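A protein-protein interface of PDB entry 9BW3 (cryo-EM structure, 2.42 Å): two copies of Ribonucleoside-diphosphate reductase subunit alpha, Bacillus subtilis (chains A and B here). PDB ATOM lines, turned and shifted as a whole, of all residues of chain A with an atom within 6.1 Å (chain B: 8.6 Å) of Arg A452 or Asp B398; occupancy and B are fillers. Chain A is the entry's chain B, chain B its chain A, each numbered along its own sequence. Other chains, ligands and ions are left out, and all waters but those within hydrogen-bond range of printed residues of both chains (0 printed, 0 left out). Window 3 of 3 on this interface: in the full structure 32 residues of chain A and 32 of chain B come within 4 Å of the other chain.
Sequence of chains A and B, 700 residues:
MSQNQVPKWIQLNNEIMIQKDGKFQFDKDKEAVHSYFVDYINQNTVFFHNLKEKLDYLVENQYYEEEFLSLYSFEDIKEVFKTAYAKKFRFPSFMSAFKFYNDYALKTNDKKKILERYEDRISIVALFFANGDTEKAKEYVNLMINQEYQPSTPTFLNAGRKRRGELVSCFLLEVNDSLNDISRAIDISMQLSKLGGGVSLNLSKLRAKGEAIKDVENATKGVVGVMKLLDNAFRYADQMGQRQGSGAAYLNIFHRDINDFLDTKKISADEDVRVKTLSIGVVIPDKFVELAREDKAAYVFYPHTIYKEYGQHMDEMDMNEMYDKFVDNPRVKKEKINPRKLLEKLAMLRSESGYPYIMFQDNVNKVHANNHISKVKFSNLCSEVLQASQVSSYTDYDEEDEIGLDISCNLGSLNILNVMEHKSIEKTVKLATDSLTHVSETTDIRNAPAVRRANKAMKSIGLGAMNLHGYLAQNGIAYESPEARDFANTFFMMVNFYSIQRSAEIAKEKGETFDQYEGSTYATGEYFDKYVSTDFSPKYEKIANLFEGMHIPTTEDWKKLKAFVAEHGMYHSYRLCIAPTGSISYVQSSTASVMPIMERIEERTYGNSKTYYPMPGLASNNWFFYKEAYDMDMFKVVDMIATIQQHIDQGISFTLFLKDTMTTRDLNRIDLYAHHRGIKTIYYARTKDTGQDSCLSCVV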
ATOM      1  N   ASP A 406     -12.393 -10.495  -0.164  1.00  0.00           N
ATOM      2  CA  ASP A 406     -11.812 -11.252   0.930  1.00  0.00           C
ATOM      3  C   ASP A 406     -12.924 -12.002   1.657  1.00  0.00           C
ATOM      4  O   ASP A 406     -14.098 -11.934   1.291  1.00  0.00           O
ATOM      5  CB  ASP A 406     -11.037 -10.330   1.872  1.00  0.00           C
ATOM      6  CG  ASP A 406      -9.598 -10.132   1.438  1.00  0.00           C
ATOM      7  OD1 ASP A 406      -9.111 -10.919   0.599  1.00  0.00           O
ATOM      8  OD2 ASP A 406      -8.953  -9.185   1.933  1.00  0.00           O
ATOM      9  N   ASP A 444     -17.450  -2.705   9.813  1.00  0.00           N
ATOM     10  CA  ASP A 444     -16.830  -1.958   8.722  1.00  0.00           C
ATOM     11  C   ASP A 444     -15.346  -1.818   9.026  1.00  0.00           C
ATOM     12  O   ASP A 444     -14.965  -1.055   9.919  1.00  0.00           O
ATOM     13  CB  ASP A 444     -17.485  -0.592   8.543  1.00  0.00           C
ATOM     14  CG  ASP A 444     -16.928   0.170   7.356  1.00  0.00           C
ATOM     15  OD1 ASP A 444     -16.044  -0.374   6.659  1.00  0.00           O
ATOM     16  OD2 ASP A 444     -17.374   1.311   7.117  1.00  0.00           O
ATOM     17  N   ILE A 445     -14.518  -2.552   8.293  1.00  0.00           N
ATOM     18  CA  ILE A 445     -13.068  -2.462   8.411  1.00  0.00           C
ATOM     19  C   ILE A 445     -12.592  -1.478   7.352  1.00  0.00           C
ATOM     20  O   ILE A 445     -12.766  -1.709   6.151  1.00  0.00           O
ATOM     21  CB  ILE A 445     -12.394  -3.832   8.250  1.00  0.00           C
ATOM     22  CG1 ILE A 445     -12.679  -4.718   9.465  1.00  0.00           C
ATOM     23  CG2 ILE A 445     -10.895  -3.667   8.062  1.00  0.00           C
ATOM     24  CD1 ILE A 445     -14.082  -5.270   9.511  1.00  0.00           C
ATOM     25  N   ARG A 446     -11.987  -0.380   7.794  1.00  0.00           N
ATOM     26  CA  ARG A 446     -11.579   0.699   6.907  1.00  0.00           C
ATOM     27  C   ARG A 446     -10.124   0.591   6.470  1.00  0.00           C
ATOM     28  O   ARG A 446      -9.601   1.531   5.861  1.00  0.00           O
ATOM     29  CB  ARG A 446     -11.828   2.051   7.580  1.00  0.00           C
ATOM     30  CG  ARG A 446     -11.384   2.115   9.029  1.00  0.00           C
ATOM     31  CD  ARG A 446     -12.199   3.134   9.809  1.00  0.00           C
ATOM     32  NE  ARG A 446     -13.598   2.740   9.930  1.00  0.00           N
ATOM     33  CZ  ARG A 446     -14.567   3.149   9.122  1.00  0.00           C
ATOM     34  NH1 ARG A 446     -14.325   3.969   8.112  1.00  0.00           N
ATOM     35  NH2 ARG A 446     -15.810   2.724   9.332  1.00  0.00           N
ATOM     36  N   ASN A 447      -9.463  -0.528   6.761  1.00  0.00           N
ATOM     37  CA  ASN A 447      -8.096  -0.759   6.323  1.00  0.00           C
ATOM     38  C   ASN A 447      -7.933  -2.071   5.570  1.00  0.00           C
ATOM     39  O   ASN A 447      -6.803  -2.443   5.239  1.00  0.00           O
ATOM     40  CB  ASN A 447      -7.141  -0.732   7.523  1.00  0.00           C
ATOM     41  CG  ASN A 447      -6.496   0.622   7.717  1.00  0.00           C
ATOM     42  OD1 ASN A 447      -6.253   1.349   6.755  1.00  0.00           O
ATOM     43  ND2 ASN A 447      -6.227   0.975   8.966  1.00  0.00           N
ATOM     44  N   ALA A 448      -9.026  -2.779   5.295  1.00  0.00           N
ATOM     45  CA  ALA A 448      -9.015  -4.006   4.501  1.00  0.00           C
ATOM     46  C   ALA A 448     -10.089  -3.863   3.432  1.00  0.00           C
ATOM     47  O   ALA A 448     -11.217  -4.344   3.599  1.00  0.00           O
ATOM     48  CB  ALA A 448      -9.245  -5.239   5.375  1.00  0.00           C
ATOM     49  N   PRO A 449      -9.774  -3.192   2.319  1.00  0.00           N
ATOM     50  CA  PRO A 449     -10.826  -2.895   1.331  1.00  0.00           C
ATOM     51  C   PRO A 449     -11.532  -4.132   0.811  1.00  0.00           C
ATOM     52  O   PRO A 449     -12.758  -4.115   0.647  1.00  0.00           O
ATOM     53  CB  PRO A 449     -10.063  -2.168   0.214  1.00  0.00           C
ATOM     54  CG  PRO A 449      -8.763  -1.768   0.812  1.00  0.00           C
ATOM     55  CD  PRO A 449      -8.443  -2.771   1.858  1.00  0.00           C
ATOM     56  N   ALA A 450     -10.793  -5.211   0.549  1.00  0.00           N
ATOM     57  CA  ALA A 450     -11.425  -6.436   0.075  1.00  0.00           C
ATOM     58  C   ALA A 450     -12.334  -7.031   1.141  1.00  0.00           C
ATOM     59  O   ALA A 450     -13.425  -7.516   0.832  1.00  0.00           O
ATOM     60  CB  ALA A 450     -10.362  -7.444  -0.359  1.00  0.00           C
ATOM     61  N   VAL A 451     -11.906  -6.992   2.404  1.00  0.00           N
ATOM     62  CA  VAL A 451     -12.729  -7.528   3.485  1.00  0.00           C
ATOM     63  C   VAL A 451     -14.021  -6.734   3.611  1.00  0.00           C
ATOM     64  O   VAL A 451     -15.112  -7.302   3.720  1.00  0.00           O
ATOM     65  CB  VAL A 451     -11.938  -7.536   4.807  1.00  0.00           C
ATOM     66  CG1 VAL A 451     -12.873  -7.760   5.983  1.00  0.00           C
ATOM     67  CG2 VAL A 451     -10.858  -8.601   4.769  1.00  0.00           C
ATOM     68  N   ARG A 452     -13.919  -5.404   3.602  1.00  0.00           N
ATOM     69  CA  ARG A 452     -15.111  -4.571   3.717  1.00  0.00           C
ATOM     70  C   ARG A 452     -16.045  -4.779   2.532  1.00  0.00           C
ATOM     71  O   ARG A 452     -17.264  -4.917   2.704  1.00  0.00           O
ATOM     72  CB  ARG A 452     -14.703  -3.103   3.841  1.00  0.00           C
ATOM     73  CG  ARG A 452     -15.794  -2.111   3.493  1.00  0.00           C
ATOM     74  CD  ARG A 452     -15.215  -0.728   3.265  1.00  0.00           C
ATOM     75  NE  ARG A 452     -15.152   0.053   4.493  1.00  0.00           N
ATOM     76  CZ  ARG A 452     -14.514   1.209   4.615  1.00  0.00           C
ATOM     77  NH1 ARG A 452     -13.873   1.756   3.595  1.00  0.00           N
ATOM     78  NH2 ARG A 452     -14.520   1.832   5.790  1.00  0.00           N
ATOM     79  N   ARG A 453     -15.488  -4.822   1.320  1.00  0.00           N
ATOM     80  CA  ARG A 453     -16.310  -5.016   0.133  1.00  0.00           C
ATOM     81  C   ARG A 453     -17.005  -6.370   0.157  1.00  0.00           C
ATOM     82  O   ARG A 453     -18.189  -6.472  -0.179  1.00  0.00           O
ATOM     83  CB  ARG A 453     -15.454  -4.874  -1.126  1.00  0.00           C
ATOM     84  CG  ARG A 453     -16.247  -4.939  -2.414  1.00  0.00           C
ATOM     85  CD  ARG A 453     -15.448  -5.562  -3.539  1.00  0.00           C
ATOM     86  NE  ARG A 453     -16.307  -5.922  -4.661  1.00  0.00           N
ATOM     87  CZ  ARG A 453     -15.936  -6.691  -5.675  1.00  0.00           C
ATOM     88  NH1 ARG A 453     -14.717  -7.199  -5.747  1.00  0.00           N
ATOM     89  NH2 ARG A 453     -16.810  -6.957  -6.640  1.00  0.00           N
ATOM     90  N   ALA A 454     -16.287  -7.423   0.554  1.00  0.00           N
ATOM     91  CA  ALA A 454     -16.881  -8.753   0.590  1.00  0.00           C
ATOM     92  C   ALA A 454     -17.929  -8.860   1.688  1.00  0.00           C
ATOM     93  O   ALA A 454     -18.942  -9.540   1.517  1.00  0.00           O
ATOM     94  CB  ALA A 454     -15.795  -9.809   0.776  1.00  0.00           C
ATOM     95  N   ASN A 455     -17.703  -8.204   2.826  1.00  0.00           N
ATOM     96  CA  ASN A 455     -18.720  -8.195   3.870  1.00  0.00           C
ATOM     97  C   ASN A 455     -19.985  -7.500   3.389  1.00  0.00           C
ATOM     98  O   ASN A 455     -21.099  -7.952   3.674  1.00  0.00           O
ATOM     99  CB  ASN A 455     -18.175  -7.521   5.129  1.00  0.00           C
ATOM    100  CG  ASN A 455     -19.231  -7.350   6.199  1.00  0.00           C
ATOM    101  OD1 ASN A 455     -19.742  -8.327   6.744  1.00  0.00           O
ATOM    102  ND2 ASN A 455     -19.570  -6.105   6.503  1.00  0.00           N
ATOM    103  N   LYS A 456     -19.832  -6.395   2.658  1.00  0.00           N
ATOM    104  CA  LYS A 456     -21.001  -5.686   2.154  1.00  0.00           C
ATOM    105  C   LYS A 456     -21.708  -6.461   1.045  1.00  0.00           C
ATOM    106  O   LYS A 456     -22.939  -6.405   0.943  1.00  0.00           O
ATOM    107  CB  LYS A 456     -20.593  -4.298   1.662  1.00  0.00           C
ATOM    108  CG  LYS A 456     -21.678  -3.556   0.906  1.00  0.00           C
ATOM    109  CD  LYS A 456     -21.084  -2.454   0.044  1.00  0.00           C
ATOM    110  CE  LYS A 456     -19.757  -2.876  -0.577  1.00  0.00           C
ATOM    111  NZ  LYS A 456     -19.870  -4.116  -1.394  1.00  0.00           N
ATOM    112  N   ALA A 457     -20.961  -7.189   0.216  1.00  0.00           N
ATOM    113  CA  ALA A 457     -21.530  -7.842  -0.959  1.00  0.00           C
ATOM    114  C   ALA A 457     -22.097  -9.228  -0.661  1.00  0.00           C
ATOM    115  O   ALA A 457     -23.191  -9.563  -1.123  1.00  0.00           O
ATOM    116  CB  ALA A 457     -20.470  -7.938  -2.062  1.00  0.00           C
ATOM    117  N   THR B 395      -2.583   7.644   5.995  1.00  0.00           N
ATOM    118  CA  THR B 395      -3.832   7.421   6.697  1.00  0.00           C
ATOM    119  C   THR B 395      -4.452   6.091   6.270  1.00  0.00           C
ATOM    120  O   THR B 395      -3.830   5.279   5.578  1.00  0.00           O
ATOM    121  CB  THR B 395      -4.775   8.599   6.449  1.00  0.00           C
ATOM    122  OG1 THR B 395      -5.078   8.684   5.052  1.00  0.00           O
ATOM    123  CG2 THR B 395      -4.125   9.896   6.894  1.00  0.00           C
ATOM    124  N   ASP B 396      -5.690   5.860   6.694  1.00  0.00           N
ATOM    125  CA  ASP B 396      -6.388   4.629   6.365  1.00  0.00           C
ATOM    126  C   ASP B 396      -6.694   4.566   4.872  1.00  0.00           C
ATOM    127  O   ASP B 396      -6.682   5.574   4.162  1.00  0.00           O
ATOM    128  CB  ASP B 396      -7.688   4.519   7.161  1.00  0.00           C
ATOM    129  CG  ASP B 396      -7.451   4.421   8.652  1.00  0.00           C
ATOM    130  OD1 ASP B 396      -6.592   3.619   9.070  1.00  0.00           O
ATOM    131  OD2 ASP B 396      -8.130   5.146   9.409  1.00  0.00           O
ATOM    132  N   TYR B 397      -6.967   3.354   4.397  1.00  0.00           N
ATOM    133  CA  TYR B 397      -7.410   3.180   3.022  1.00  0.00           C
ATOM    134  C   TYR B 397      -8.668   4.002   2.774  1.00  0.00           C
ATOM    135  O   TYR B 397      -9.551   4.091   3.631  1.00  0.00           O
ATOM    136  CB  TYR B 397      -7.678   1.703   2.731  1.00  0.00           C
ATOM    137  CG  TYR B 397      -7.640   1.351   1.262  1.00  0.00           C
ATOM    138  CD1 TYR B 397      -6.461   0.937   0.657  1.00  0.00           C
ATOM    139  CD2 TYR B 397      -8.782   1.439   0.477  1.00  0.00           C
ATOM    140  CE1 TYR B 397      -6.422   0.615  -0.682  1.00  0.00           C
ATOM    141  CE2 TYR B 397      -8.752   1.120  -0.864  1.00  0.00           C
ATOM    142  CZ  TYR B 397      -7.570   0.708  -1.438  1.00  0.00           C
ATOM    143  OH  TYR B 397      -7.534   0.390  -2.774  1.00  0.00           O
ATOM    144  N   ASP B 398      -8.745   4.607   1.593  1.00  0.00           N
ATOM    145  CA  ASP B 398      -9.811   5.512   1.172  1.00  0.00           C
ATOM    146  C   ASP B 398      -9.645   6.894   1.792  1.00  0.00           C
ATOM    147  O   ASP B 398     -10.427   7.796   1.468  1.00  0.00           O
ATOM    148  CB  ASP B 398     -11.214   4.982   1.505  1.00  0.00           C
ATOM    149  CG  ASP B 398     -11.542   3.697   0.771  1.00  0.00           C
ATOM    150  OD1 ASP B 398     -11.358   3.654  -0.464  1.00  0.00           O
ATOM    151  OD2 ASP B 398     -11.985   2.732   1.428  1.00  0.00           O
ATOM    152  N   GLU B 399      -8.666   7.094   2.669  1.00  0.00           N
ATOM    153  CA  GLU B 399      -8.357   8.404   3.225  1.00  0.00           C
ATOM    154  C   GLU B 399      -7.151   8.982   2.497  1.00  0.00           C
ATOM    155  O   GLU B 399      -6.177   8.267   2.237  1.00  0.00           O
ATOM    156  CB  GLU B 399      -8.074   8.311   4.724  1.00  0.00           C
ATOM    157  CG  GLU B 399      -9.211   8.791   5.607  1.00  0.00           C
ATOM    158  CD  GLU B 399      -8.761   9.078   7.026  1.00  0.00           C
ATOM    159  OE1 GLU B 399      -8.848   8.169   7.878  1.00  0.00           O
ATOM    160  OE2 GLU B 399      -8.316  10.216   7.291  1.00  0.00           O
ATOM    161  N   GLU B 400      -7.223  10.268   2.163  1.00  0.00           N
ATOM    162  CA  GLU B 400      -6.107  10.923   1.495  1.00  0.00           C
ATOM    163  C   GLU B 400      -4.882  10.947   2.400  1.00  0.00           C
ATOM    164  O   GLU B 400      -4.981  11.207   3.602  1.00  0.00           O
ATOM    165  CB  GLU B 400      -6.487  12.348   1.092  1.00  0.00           C
ATOM    166  CG  GLU B 400      -7.245  12.447  -0.222  1.00  0.00           C
ATOM    167  CD  GLU B 400      -6.898  11.326  -1.181  1.00  0.00           C
ATOM    168  OE1 GLU B 400      -5.883  11.444  -1.898  1.00  0.00           O
ATOM    169  OE2 GLU B 400      -7.644  10.325  -1.220  1.00  0.00           O
ATOM    170  N   ASP B 401      -3.722  10.672   1.814  1.00  0.00           N
ATOM    171  CA  ASP B 401      -2.462  10.718   2.537  1.00  0.00           C
ATOM    172  C   ASP B 401      -1.885  12.126   2.512  1.00  0.00           C
ATOM    173  O   ASP B 401      -2.098  12.890   1.567  1.00  0.00           O
ATOM    174  CB  ASP B 401      -1.454   9.737   1.937  1.00  0.00           C
ATOM    175  CG  ASP B 401      -1.813   8.291   2.208  1.00  0.00           C
ATOM    176  OD1 ASP B 401      -2.404   8.012   3.270  1.00  0.00           O
ATOM    177  OD2 ASP B 401      -1.498   7.432   1.359  1.00  0.00           O
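Among the printed residues, pairs that only touch across the chains: Arg A446 with Asp B396 and Pro A449 with Tyr B397.
OD2 of Asp B398 lies within salt-bridge range of NH1 of Arg A452 (3.0 Å).
O of Tyr B397 lies close to O of Arg A446.
OD1 of Asn A447 lies within hydrogen-bond range of N of Tyr B397, 3.2 Å away.
OD1 of Asp B396 is in hydrogen-bond range of ND2 of Asn A447.
Of the 7 printed residues of chain B, 3 touch a printed residue of chain A.
Printed residues of chain A that touch a printed residue of chain B: Arg A446, Asn A447, Pro A449 and Arg A452.
Hydrophobic or aromatic side chains of chain A that line the printed part of chain B: Pro A449.
Along chain A the printed residues that touch a printed residue of chain B span positions 446 to 452.
Asp B398 touches just one residue of chain A: Arg A452 (3.0 Å).
Of the printed residues of chain B, Arg A446 touches Asp B396 (3.8 Å) and Tyr B397 (3.4 Å).
Printed residues of chain B within 4 Å of Asn A447: Asp B396 and Tyr B397.
Of the printed residues of chain A, Tyr B397 touches Arg A446 (3.4 Å), Asn A447 (3.2 Å) and Pro A449 (3.2 Å).
The nearest residue of chain B that does not touch Arg A452 is Tyr B397 (4.9 Å).
The nearest printed residue of chain B that does not touch Pro A449 is Asp B398 (5.4 Å).
The backbone carbonyl oxygen of Ile A445 lies close to the guanidinium group of Arg A452, 3.4 Å away.
The side-chain carboxylate (OD2) of Asp A444 is in salt-bridge range of the guanidinium group (NH2) of Arg A446.
OD1 of Asp A444 lies within salt-bridge range of NH2 of Arg A452 (2.8 Å).
No position is printed for both chains.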
